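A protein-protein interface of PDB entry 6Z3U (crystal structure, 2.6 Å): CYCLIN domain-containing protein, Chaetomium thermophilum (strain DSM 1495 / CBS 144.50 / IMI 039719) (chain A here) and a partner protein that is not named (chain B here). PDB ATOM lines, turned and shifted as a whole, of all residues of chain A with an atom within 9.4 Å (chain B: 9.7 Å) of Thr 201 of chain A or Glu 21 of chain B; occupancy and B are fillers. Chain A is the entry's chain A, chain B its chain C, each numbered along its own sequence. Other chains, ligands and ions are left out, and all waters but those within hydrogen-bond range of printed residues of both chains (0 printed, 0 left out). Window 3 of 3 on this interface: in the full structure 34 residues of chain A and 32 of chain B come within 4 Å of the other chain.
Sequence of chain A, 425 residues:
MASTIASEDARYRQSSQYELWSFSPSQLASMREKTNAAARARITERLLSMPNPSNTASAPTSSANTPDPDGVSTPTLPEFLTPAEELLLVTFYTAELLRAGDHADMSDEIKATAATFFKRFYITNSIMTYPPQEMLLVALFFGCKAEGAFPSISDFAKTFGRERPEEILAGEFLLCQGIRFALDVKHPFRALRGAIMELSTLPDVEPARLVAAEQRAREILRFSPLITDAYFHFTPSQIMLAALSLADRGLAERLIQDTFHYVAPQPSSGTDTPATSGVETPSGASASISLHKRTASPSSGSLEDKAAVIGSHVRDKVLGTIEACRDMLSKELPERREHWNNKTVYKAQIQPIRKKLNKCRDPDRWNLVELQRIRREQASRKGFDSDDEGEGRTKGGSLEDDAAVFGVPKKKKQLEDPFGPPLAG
CD2 of His 24 of chain B touches CG2 of Ile 196 of chain A (3.9 Å).
O of Met 197 of chain A touches CD2 of Leu 22 of chain B (3.7 Å).
CG of Met 197 of chain A touches O of Asn 23 of chain B (3.4 Å).
Met 197 of chain A touches His 24 of chain B (CG to CB, 3.9 Å).
Glu 198 of chain A touches Met 51 of chain B (OE1 to CE, 3.8 Å).
Thr 201 of chain A touches Glu 21 of chain B.
Leu 22 of chain B touches Thr 201 of chain A (CD2 to CG2, 3.9 Å).
OD1 of Asp 28 of chain B lies within hydrogen-bond range of ND2 of Asn 23 of chain B (3.1 Å).
The side-chain hydroxyl of Thr 201 of chain A is in hydrogen-bond range of the backbone carbonyl oxygen of Glu 198 of chain A, at 2.7 Å.
The backbone carbonyl oxygen (O) of Arg 17 of chain B lies within hydrogen-bond range of the guanidinium group (NH2) of Arg 19 of chain B (3.5 Å).
The side-chain hydroxyl (OG) of Ser 200 of chain A is in hydrogen-bond range of the backbone carbonyl oxygen (O) of Ile 196 of chain A, at 3.0 Å.
The side-chain amide oxygen of Asn 23 of chain B is in hydrogen-bond range of the guanidinium group of Arg 31 of chain B (2.7 Å).
The guanidinium group of Arg 19 of chain B sits at hydrogen-bond distance from the side-chain hydroxyl of Thr 201 of chain A (3.3 Å).
The side-chain sulfur of Met 51 of chain B lies close to the backbone carbonyl oxygen of Gly 194 of chain A, 3.4 Å away.
The guanidinium group (NH2) of Arg 19 of chain B is in salt-bridge range of the side-chain carboxylate (OE1) of Glu 198 of chain A, 2.5 Å away.
Thr 201 of chain A touches three residues of chain B.
Glu 21 of chain B touches one residue of chain A.
Of the printed residues of chain B, Glu 198 of chain A touches Arg 19 and Met 51.
No residue of chain B comes within 4 Å of Ser 200 of chain A.
Of the printed residues of chain A, His 24 of chain B touches Ile 196 and Met 197.
Printed residues of chain B within 4 Å of Gly 194 of chain A: Met 51 (3.4 Å).
Of the printed residues of chain B, Ile 196 of chain A touches His 24 (3.9 Å).
Arg 254 of chain A touches none of the printed residues of chain B.
Leu 44 of chain B touches none of the printed residues of chain A.
The nearest residue of chain A that does not touch Glu 21 of chain B is Ser 200 of chain A (5.9 Å).
The nearest printed residue of chain A that does not touch Leu 22 of chain B is Glu 198 of chain A (4.1 Å).
Along chain B the printed residues that touch a printed residue of chain A span positions 19 to 51.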
ATOM      1  N   GLY A 194       5.608 -17.353  -6.054  1.00  0.00           N
ATOM      2  CA  GLY A 194       7.042 -17.582  -6.039  1.00  0.00           C
ATOM      3  C   GLY A 194       7.609 -17.789  -7.429  1.00  0.00           C
ATOM      4  O   GLY A 194       8.703 -17.309  -7.743  1.00  0.00           O
ATOM      5  N   ALA A 195       6.871 -18.498  -8.286  1.00  0.00           N
ATOM      6  CA  ALA A 195       7.335 -18.734  -9.647  1.00  0.00           C
ATOM      7  C   ALA A 195       7.356 -17.454 -10.472  1.00  0.00           C
ATOM      8  O   ALA A 195       8.191 -17.316 -11.373  1.00  0.00           O
ATOM      9  CB  ALA A 195       6.452 -19.781 -10.326  1.00  0.00           C
ATOM     10  N   ILE A 196       6.457 -16.510 -10.184  1.00  0.00           N
ATOM     11  CA  ILE A 196       6.435 -15.259 -10.936  1.00  0.00           C
ATOM     12  C   ILE A 196       7.689 -14.440 -10.657  1.00  0.00           C
ATOM     13  O   ILE A 196       8.246 -13.806 -11.561  1.00  0.00           O
ATOM     14  CB  ILE A 196       5.160 -14.460 -10.609  1.00  0.00           C
ATOM     15  CG1 ILE A 196       3.918 -15.196 -11.117  1.00  0.00           C
ATOM     16  CG2 ILE A 196       5.240 -13.058 -11.203  1.00  0.00           C
ATOM     17  CD1 ILE A 196       3.841 -15.324 -12.628  1.00  0.00           C
ATOM     18  N   MET A 197       8.153 -14.431  -9.406  1.00  0.00           N
ATOM     19  CA  MET A 197       9.345 -13.655  -9.077  1.00  0.00           C
ATOM     20  C   MET A 197      10.570 -14.185  -9.811  1.00  0.00           C
ATOM     21  O   MET A 197      11.395 -13.402 -10.296  1.00  0.00           O
ATOM     22  CB  MET A 197       9.567 -13.645  -7.566  1.00  0.00           C
ATOM     23  CG  MET A 197       8.515 -12.835  -6.824  1.00  0.00           C
ATOM     24  SD  MET A 197       8.687 -12.853  -5.033  1.00  0.00           S
ATOM     25  CE  MET A 197       8.276 -14.552  -4.646  1.00  0.00           C
ATOM     26  N   GLU A 198      10.713 -15.510  -9.904  1.00  0.00           N
ATOM     27  CA  GLU A 198      11.836 -16.067 -10.652  1.00  0.00           C
ATOM     28  C   GLU A 198      11.790 -15.627 -12.112  1.00  0.00           C
ATOM     29  O   GLU A 198      12.835 -15.387 -12.729  1.00  0.00           O
ATOM     30  CB  GLU A 198      11.836 -17.592 -10.547  1.00  0.00           C
ATOM     31  CG  GLU A 198      12.948 -18.273 -11.340  1.00  0.00           C
ATOM     32  CD  GLU A 198      14.335 -17.824 -10.922  1.00  0.00           C
ATOM     33  OE1 GLU A 198      14.579 -17.698  -9.705  1.00  0.00           O
ATOM     34  OE2 GLU A 198      15.178 -17.595 -11.816  1.00  0.00           O
ATOM     35  N   LEU A 199      10.585 -15.511 -12.680  1.00  0.00           N
ATOM     36  CA  LEU A 199      10.454 -15.036 -14.053  1.00  0.00           C
ATOM     37  C   LEU A 199      10.723 -13.539 -14.157  1.00  0.00           C
ATOM     38  O   LEU A 199      11.264 -13.077 -15.169  1.00  0.00           O
ATOM     39  CB  LEU A 199       9.059 -15.355 -14.592  1.00  0.00           C
ATOM     40  CG  LEU A 199       8.758 -16.823 -14.891  1.00  0.00           C
ATOM     41  CD1 LEU A 199       7.258 -17.065 -14.928  1.00  0.00           C
ATOM     42  CD2 LEU A 199       9.397 -17.229 -16.213  1.00  0.00           C
ATOM     43  N   SER A 200      10.363 -12.771 -13.127  1.00  0.00           N
ATOM     44  CA  SER A 200      10.580 -11.331 -13.164  1.00  0.00           C
ATOM     45  C   SER A 200      12.054 -10.976 -13.298  1.00  0.00           C
ATOM     46  O   SER A 200      12.376  -9.858 -13.715  1.00  0.00           O
ATOM     47  CB  SER A 200      10.003 -10.685 -11.904  1.00  0.00           C
ATOM     48  OG  SER A 200       8.599 -10.851 -11.844  1.00  0.00           O
ATOM     49  N   THR A 201      12.956 -11.899 -12.957  1.00  0.00           N
ATOM     50  CA  THR A 201      14.384 -11.639 -13.079  1.00  0.00           C
ATOM     51  C   THR A 201      14.866 -11.702 -14.523  1.00  0.00           C
ATOM     52  O   THR A 201      15.939 -11.168 -14.826  1.00  0.00           O
ATOM     53  CB  THR A 201      15.179 -12.638 -12.230  1.00  0.00           C
ATOM     54  OG1 THR A 201      15.076 -13.950 -12.797  1.00  0.00           O
ATOM     55  CG2 THR A 201      14.653 -12.662 -10.800  1.00  0.00           C
ATOM     56  N   LEU A 202      14.109 -12.335 -15.408  1.00  0.00           N
ATOM     57  CA  LEU A 202      14.488 -12.390 -16.818  1.00  0.00           C
ATOM     58  C   LEU A 202      14.227 -11.036 -17.471  1.00  0.00           C
ATOM     59  O   LEU A 202      13.147 -10.464 -17.286  1.00  0.00           O
ATOM     60  CB  LEU A 202      13.703 -13.489 -17.531  1.00  0.00           C
ATOM     61  CG  LEU A 202      14.219 -14.923 -17.387  1.00  0.00           C
ATOM     62  CD1 LEU A 202      14.496 -15.285 -15.937  1.00  0.00           C
ATOM     63  CD2 LEU A 202      13.217 -15.898 -17.990  1.00  0.00           C
ATOM     64  N   PRO A 203      15.185 -10.482 -18.232  1.00  0.00           N
ATOM     65  CA  PRO A 203      14.961  -9.165 -18.848  1.00  0.00           C
ATOM     66  C   PRO A 203      14.110  -9.202 -20.108  1.00  0.00           C
ATOM     67  O   PRO A 203      13.456  -8.210 -20.447  1.00  0.00           O
ATOM     68  CB  PRO A 203      16.385  -8.687 -19.165  1.00  0.00           C
ATOM     69  CG  PRO A 203      17.152  -9.946 -19.384  1.00  0.00           C
ATOM     70  CD  PRO A 203      16.564 -10.964 -18.444  1.00  0.00           C
ATOM     71  N   ASP A 204      14.107 -10.337 -20.813  1.00  0.00           N
ATOM     72  CA  ASP A 204      13.341 -10.430 -22.052  1.00  0.00           C
ATOM     73  C   ASP A 204      11.840 -10.527 -21.793  1.00  0.00           C
ATOM     74  O   ASP A 204      11.041 -10.073 -22.622  1.00  0.00           O
ATOM     75  CB  ASP A 204      13.818 -11.620 -22.895  1.00  0.00           C
ATOM     76  CG  ASP A 204      14.129 -12.851 -22.064  1.00  0.00           C
ATOM     77  OD1 ASP A 204      14.213 -12.731 -20.824  1.00  0.00           O
ATOM     78  OD2 ASP A 204      14.296 -13.939 -22.654  1.00  0.00           O
ATOM     79  N   VAL A 205      11.434 -11.110 -20.662  1.00  0.00           N
ATOM     80  CA  VAL A 205      10.014 -11.267 -20.372  1.00  0.00           C
ATOM     81  C   VAL A 205       9.384  -9.903 -20.106  1.00  0.00           C
ATOM     82  O   VAL A 205      10.012  -8.997 -19.543  1.00  0.00           O
ATOM     83  CB  VAL A 205       9.796 -12.212 -19.175  1.00  0.00           C
ATOM     84  CG1 VAL A 205      10.611 -13.487 -19.340  1.00  0.00           C
ATOM     85  CG2 VAL A 205      10.140 -11.507 -17.873  1.00  0.00           C
ATOM     86  N   GLU A 206       8.121  -9.761 -20.508  1.00  0.00           N
ATOM     87  CA  GLU A 206       7.379  -8.512 -20.381  1.00  0.00           C
ATOM     88  C   GLU A 206       6.534  -8.521 -19.113  1.00  0.00           C
ATOM     89  O   GLU A 206       5.887  -9.528 -18.808  1.00  0.00           O
ATOM     90  CB  GLU A 206       6.474  -8.320 -21.602  1.00  0.00           C
ATOM     91  CG  GLU A 206       5.437  -7.198 -21.504  1.00  0.00           C
ATOM     92  CD  GLU A 206       6.015  -5.827 -21.787  1.00  0.00           C
ATOM     93  OE1 GLU A 206       6.909  -5.718 -22.652  1.00  0.00           O
ATOM     94  OE2 GLU A 206       5.573  -4.857 -21.136  1.00  0.00           O
ATOM     95  N   LEU A 210       3.486 -11.090 -17.829  1.00  0.00           N
ATOM     96  CA  LEU A 210       3.580 -11.831 -16.574  1.00  0.00           C
ATOM     97  C   LEU A 210       2.317 -11.666 -15.740  1.00  0.00           C
ATOM     98  O   LEU A 210       1.816 -12.636 -15.160  1.00  0.00           O
ATOM     99  CB  LEU A 210       4.800 -11.367 -15.779  1.00  0.00           C
ATOM    100  CG  LEU A 210       6.083 -12.186 -15.918  1.00  0.00           C
ATOM    101  CD1 LEU A 210       7.177 -11.600 -15.035  1.00  0.00           C
ATOM    102  CD2 LEU A 210       5.844 -13.649 -15.574  1.00  0.00           C
ATOM    103  N   ARG A 254       9.833 -21.901 -20.163  1.00  0.00           N
ATOM    104  CA  ARG A 254      11.021 -21.103 -19.878  1.00  0.00           C
ATOM    105  C   ARG A 254      11.564 -21.411 -18.489  1.00  0.00           C
ATOM    106  O   ARG A 254      12.767 -21.641 -18.313  1.00  0.00           O
ATOM    107  CB  ARG A 254      10.690 -19.614 -20.003  1.00  0.00           C
ATOM    108  CG  ARG A 254      11.846 -18.675 -19.678  1.00  0.00           C
ATOM    109  CD  ARG A 254      13.112 -19.036 -20.438  1.00  0.00           C
ATOM    110  NE  ARG A 254      14.160 -18.035 -20.256  1.00  0.00           N
ATOM    111  CZ  ARG A 254      14.235 -16.893 -20.932  1.00  0.00           C
ATOM    112  NH1 ARG A 254      15.229 -16.048 -20.693  1.00  0.00           N
ATOM    113  NH2 ARG A 254      13.316 -16.586 -21.839  1.00  0.00           N
ATOM    114  N   LEU A 255      10.683 -21.436 -17.489  1.00  0.00           N
ATOM    115  CA  LEU A 255      11.127 -21.631 -16.112  1.00  0.00           C
ATOM    116  C   LEU A 255      11.773 -23.000 -15.929  1.00  0.00           C
ATOM    117  O   LEU A 255      12.800 -23.124 -15.249  1.00  0.00           O
ATOM    118  CB  LEU A 255       9.935 -21.456 -15.170  1.00  0.00           C
ATOM    119  CG  LEU A 255      10.199 -21.112 -13.704  1.00  0.00           C
ATOM    120  CD1 LEU A 255      11.201 -19.976 -13.584  1.00  0.00           C
ATOM    121  CD2 LEU A 255       8.890 -20.739 -13.022  1.00  0.00           C
ATOM    122  N   ASP A 258      15.294 -23.145 -17.684  1.00  0.00           N
ATOM    123  CA  ASP A 258      16.341 -22.373 -17.023  1.00  0.00           C
ATOM    124  C   ASP A 258      16.956 -23.143 -15.860  1.00  0.00           C
ATOM    125  O   ASP A 258      18.184 -23.240 -15.743  1.00  0.00           O
ATOM    126  CB  ASP A 258      15.775 -21.035 -16.540  1.00  0.00           C
ATOM    127  CG  ASP A 258      15.746 -19.980 -17.633  1.00  0.00           C
ATOM    128  OD1 ASP A 258      16.074 -20.306 -18.795  1.00  0.00           O
ATOM    129  OD2 ASP A 258      15.394 -18.821 -17.327  1.00  0.00           O
ATOM    130  N   ARG B  17      17.590 -20.711  -5.752  1.00  0.00           N
ATOM    131  CA  ARG B  17      18.310 -19.877  -4.800  1.00  0.00           C
ATOM    132  C   ARG B  17      17.519 -18.603  -4.548  1.00  0.00           C
ATOM    133  O   ARG B  17      17.091 -17.936  -5.494  1.00  0.00           O
ATOM    134  CB  ARG B  17      19.718 -19.567  -5.321  1.00  0.00           C
ATOM    135  CG  ARG B  17      19.740 -18.911  -6.696  1.00  0.00           C
ATOM    136  CD  ARG B  17      21.148 -18.914  -7.281  1.00  0.00           C
ATOM    137  NE  ARG B  17      21.222 -18.229  -8.570  1.00  0.00           N
ATOM    138  CZ  ARG B  17      21.017 -18.824  -9.744  1.00  0.00           C
ATOM    139  NH1 ARG B  17      20.727 -20.118  -9.801  1.00  0.00           N
ATOM    140  NH2 ARG B  17      21.106 -18.124 -10.868  1.00  0.00           N
ATOM    141  N   VAL B  18      17.331 -18.273  -3.271  1.00  0.00           N
ATOM    142  CA  VAL B  18      16.557 -17.105  -2.863  1.00  0.00           C
ATOM    143  C   VAL B  18      17.529 -15.933  -2.781  1.00  0.00           C
ATOM    144  O   VAL B  18      18.275 -15.797  -1.810  1.00  0.00           O
ATOM    145  CB  VAL B  18      15.836 -17.339  -1.534  1.00  0.00           C
ATOM    146  CG1 VAL B  18      15.162 -16.060  -1.054  1.00  0.00           C
ATOM    147  CG2 VAL B  18      14.817 -18.461  -1.670  1.00  0.00           C
ATOM    148  N   ARG B  19      17.510 -15.076  -3.796  1.00  0.00           N
ATOM    149  CA  ARG B  19      18.413 -13.938  -3.877  1.00  0.00           C
ATOM    150  C   ARG B  19      17.668 -12.641  -3.584  1.00  0.00           C
ATOM    151  O   ARG B  19      16.436 -12.589  -3.534  1.00  0.00           O
ATOM    152  CB  ARG B  19      19.106 -13.876  -5.248  1.00  0.00           C
ATOM    153  CG  ARG B  19      18.213 -14.090  -6.464  1.00  0.00           C
ATOM    154  CD  ARG B  19      18.669 -15.295  -7.286  1.00  0.00           C
ATOM    155  NE  ARG B  19      18.291 -15.181  -8.694  1.00  0.00           N
ATOM    156  CZ  ARG B  19      17.193 -15.708  -9.233  1.00  0.00           C
ATOM    157  NH1 ARG B  19      16.955 -15.540 -10.526  1.00  0.00           N
ATOM    158  NH2 ARG B  19      16.338 -16.400  -8.491  1.00  0.00           N
ATOM    159  N   GLU B  20      18.458 -11.584  -3.378  1.00  0.00           N
ATOM    160  CA  GLU B  20      17.920 -10.314  -2.904  1.00  0.00           C
ATOM    161  C   GLU B  20      17.022  -9.646  -3.937  1.00  0.00           C
ATOM    162  O   GLU B  20      16.139  -8.861  -3.568  1.00  0.00           O
ATOM    163  CB  GLU B  20      19.078  -9.387  -2.523  1.00  0.00           C
ATOM    164  CG  GLU B  20      18.672  -8.000  -2.051  1.00  0.00           C
ATOM    165  CD  GLU B  20      19.873  -7.140  -1.690  1.00  0.00           C
ATOM    166  OE1 GLU B  20      19.845  -5.922  -1.969  1.00  0.00           O
ATOM    167  OE2 GLU B  20      20.855  -7.685  -1.138  1.00  0.00           O
ATOM    168  N   GLU B  21      17.224  -9.932  -5.224  1.00  0.00           N
ATOM    169  CA  GLU B  21      16.480  -9.241  -6.268  1.00  0.00           C
ATOM    170  C   GLU B  21      15.037  -9.715  -6.398  1.00  0.00           C
ATOM    171  O   GLU B  21      14.255  -9.069  -7.103  1.00  0.00           O
ATOM    172  CB  GLU B  21      17.181  -9.414  -7.619  1.00  0.00           C
ATOM    173  CG  GLU B  21      17.118 -10.830  -8.172  1.00  0.00           C
ATOM    174  CD  GLU B  21      17.899 -10.991  -9.461  1.00  0.00           C
ATOM    175  OE1 GLU B  21      19.124 -11.232  -9.391  1.00  0.00           O
ATOM    176  OE2 GLU B  21      17.287 -10.878 -10.545  1.00  0.00           O
ATOM    177  N   LEU B  22      14.663 -10.813  -5.747  1.00  0.00           N
ATOM    178  CA  LEU B  22      13.299 -11.311  -5.851  1.00  0.00           C
ATOM    179  C   LEU B  22      12.331 -10.358  -5.158  1.00  0.00           C
ATOM    180  O   LEU B  22      12.551  -9.957  -4.011  1.00  0.00           O
ATOM    181  CB  LEU B  22      13.198 -12.707  -5.238  1.00  0.00           C
ATOM    182  CG  LEU B  22      14.022 -13.799  -5.923  1.00  0.00           C
ATOM    183  CD1 LEU B  22      13.950 -15.097  -5.139  1.00  0.00           C
ATOM    184  CD2 LEU B  22      13.549 -14.017  -7.351  1.00  0.00           C
ATOM    185  N   ASN B  23      11.260  -9.993  -5.859  1.00  0.00           N
ATOM    186  CA  ASN B  23      10.198  -9.178  -5.284  1.00  0.00           C
ATOM    187  C   ASN B  23       8.995  -9.231  -6.213  1.00  0.00           C
ATOM    188  O   ASN B  23       9.115  -9.564  -7.395  1.00  0.00           O
ATOM    189  CB  ASN B  23      10.643  -7.728  -5.066  1.00  0.00           C
ATOM    190  CG  ASN B  23       9.708  -6.964  -4.143  1.00  0.00           C
ATOM    191  OD1 ASN B  23       8.988  -7.559  -3.344  1.00  0.00           O
ATOM    192  ND2 ASN B  23       9.709  -5.642  -4.256  1.00  0.00           N
ATOM    193  N   HIS B  24       7.831  -8.885  -5.659  1.00  0.00           N
ATOM    194  CA  HIS B  24       6.565  -8.933  -6.378  1.00  0.00           C
ATOM    195  C   HIS B  24       5.806  -7.651  -6.050  1.00  0.00           C
ATOM    196  O   HIS B  24       5.731  -7.266  -4.868  1.00  0.00           O
ATOM    197  CB  HIS B  24       5.752 -10.168  -5.978  1.00  0.00           C
ATOM    198  CG  HIS B  24       4.547 -10.406  -6.831  1.00  0.00           C
ATOM    199  ND1 HIS B  24       3.393  -9.662  -6.716  1.00  0.00           N
ATOM    200  CD2 HIS B  24       4.312 -11.314  -7.808  1.00  0.00           C
ATOM    201  CE1 HIS B  24       2.501 -10.096  -7.589  1.00  0.00           C
ATOM    202  NE2 HIS B  24       3.034 -11.099  -8.264  1.00  0.00           N
ATOM    203  N   PRO B  25       5.233  -6.970  -7.047  1.00  0.00           N
ATOM    204  CA  PRO B  25       4.613  -5.663  -6.765  1.00  0.00           C
ATOM    205  C   PRO B  25       3.508  -5.728  -5.728  1.00  0.00           C
ATOM    206  O   PRO B  25       3.237  -4.725  -5.059  1.00  0.00           O
ATOM    207  CB  PRO B  25       4.081  -5.222  -8.136  1.00  0.00           C
ATOM    208  CG  PRO B  25       3.948  -6.484  -8.923  1.00  0.00           C
ATOM    209  CD  PRO B  25       5.058  -7.371  -8.453  1.00  0.00           C
ATOM    210  N   LEU B  27       3.721  -7.120  -2.991  1.00  0.00           N
ATOM    211  CA  LEU B  27       4.360  -6.914  -1.695  1.00  0.00           C
ATOM    212  C   LEU B  27       4.589  -5.437  -1.410  1.00  0.00           C
ATOM    213  O   LEU B  27       4.540  -5.016  -0.249  1.00  0.00           O
ATOM    214  CB  LEU B  27       5.693  -7.658  -1.636  1.00  0.00           C
ATOM    215  CG  LEU B  27       5.655  -9.180  -1.521  1.00  0.00           C
ATOM    216  CD1 LEU B  27       7.068  -9.739  -1.512  1.00  0.00           C
ATOM    217  CD2 LEU B  27       4.909  -9.602  -0.269  1.00  0.00           C
ATOM    218  N   ASP B  28       4.839  -4.642  -2.453  1.00  0.00           N
ATOM    219  CA  ASP B  28       5.175  -3.236  -2.263  1.00  0.00           C
ATOM    220  C   ASP B  28       4.172  -2.518  -1.370  1.00  0.00           C
ATOM    221  O   ASP B  28       4.552  -1.628  -0.600  1.00  0.00           O
ATOM    222  CB  ASP B  28       5.266  -2.539  -3.624  1.00  0.00           C
ATOM    223  CG  ASP B  28       6.313  -3.164  -4.531  1.00  0.00           C
ATOM    224  OD1 ASP B  28       7.117  -3.985  -4.035  1.00  0.00           O
ATOM    225  OD2 ASP B  28       6.329  -2.835  -5.737  1.00  0.00           O
ATOM    226  N   ARG B  31       5.207  -3.509   2.347  1.00  0.00           N
ATOM    227  CA  ARG B  31       6.535  -3.114   2.804  1.00  0.00           C
ATOM    228  C   ARG B  31       6.530  -1.704   3.380  1.00  0.00           C
ATOM    229  O   ARG B  31       7.333  -1.393   4.267  1.00  0.00           O
ATOM    230  CB  ARG B  31       7.540  -3.209   1.654  1.00  0.00           C
ATOM    231  CG  ARG B  31       7.582  -4.566   0.968  1.00  0.00           C
ATOM    232  CD  ARG B  31       8.760  -4.672   0.010  1.00  0.00           C
ATOM    233  NE  ARG B  31       9.851  -5.463   0.578  1.00  0.00           N
ATOM    234  CZ  ARG B  31      10.156  -6.712   0.222  1.00  0.00           C
ATOM    235  NH1 ARG B  31       9.464  -7.341  -0.720  1.00  0.00           N
ATOM    236  NH2 ARG B  31      11.168  -7.332   0.812  1.00  0.00           N
ATOM    237  N   LEU B  44      11.267 -11.361   3.786  1.00  0.00           N
ATOM    238  CA  LEU B  44      12.233 -12.340   3.303  1.00  0.00           C
ATOM    239  C   LEU B  44      11.732 -13.756   3.559  1.00  0.00           C
ATOM    240  O   LEU B  44      11.900 -14.646   2.717  1.00  0.00           O
ATOM    241  CB  LEU B  44      13.590 -12.130   3.976  1.00  0.00           C
ATOM    242  CG  LEU B  44      14.075 -10.704   4.264  1.00  0.00           C
ATOM    243  CD1 LEU B  44      13.663  -9.714   3.171  1.00  0.00           C
ATOM    244  CD2 LEU B  44      13.602 -10.229   5.644  1.00  0.00           C
ATOM    245  N   ILE B  47       9.072 -14.649   0.871  1.00  0.00           N
ATOM    246  CA  ILE B  47       9.704 -14.987  -0.401  1.00  0.00           C
ATOM    247  C   ILE B  47      10.353 -16.360  -0.316  1.00  0.00           C
ATOM    248  O   ILE B  47      10.233 -17.182  -1.234  1.00  0.00           O
ATOM    249  CB  ILE B  47      10.729 -13.905  -0.793  1.00  0.00           C
ATOM    250  CG1 ILE B  47      10.039 -12.549  -0.971  1.00  0.00           C
ATOM    251  CG2 ILE B  47      11.467 -14.312  -2.063  1.00  0.00           C
ATOM    252  CD1 ILE B  47      10.997 -11.383  -1.145  1.00  0.00           C
ATOM    253  N   MET B  51       9.258 -19.601  -2.701  1.00  0.00           N
ATOM    254  CA  MET B  51      10.229 -20.262  -3.568  1.00  0.00           C
ATOM    255  C   MET B  51      10.364 -21.742  -3.231  1.00  0.00           C
ATOM    256  O   MET B  51      10.487 -22.582  -4.130  1.00  0.00           O
ATOM    257  CB  MET B  51      11.582 -19.561  -3.456  1.00  0.00           C
ATOM    258  CG  MET B  51      11.598 -18.159  -4.043  1.00  0.00           C
ATOM    259  SD  MET B  51      11.439 -18.147  -5.838  1.00  0.00           S
ATOM    260  CE  MET B  51      13.127 -18.496  -6.327  1.00  0.00           C
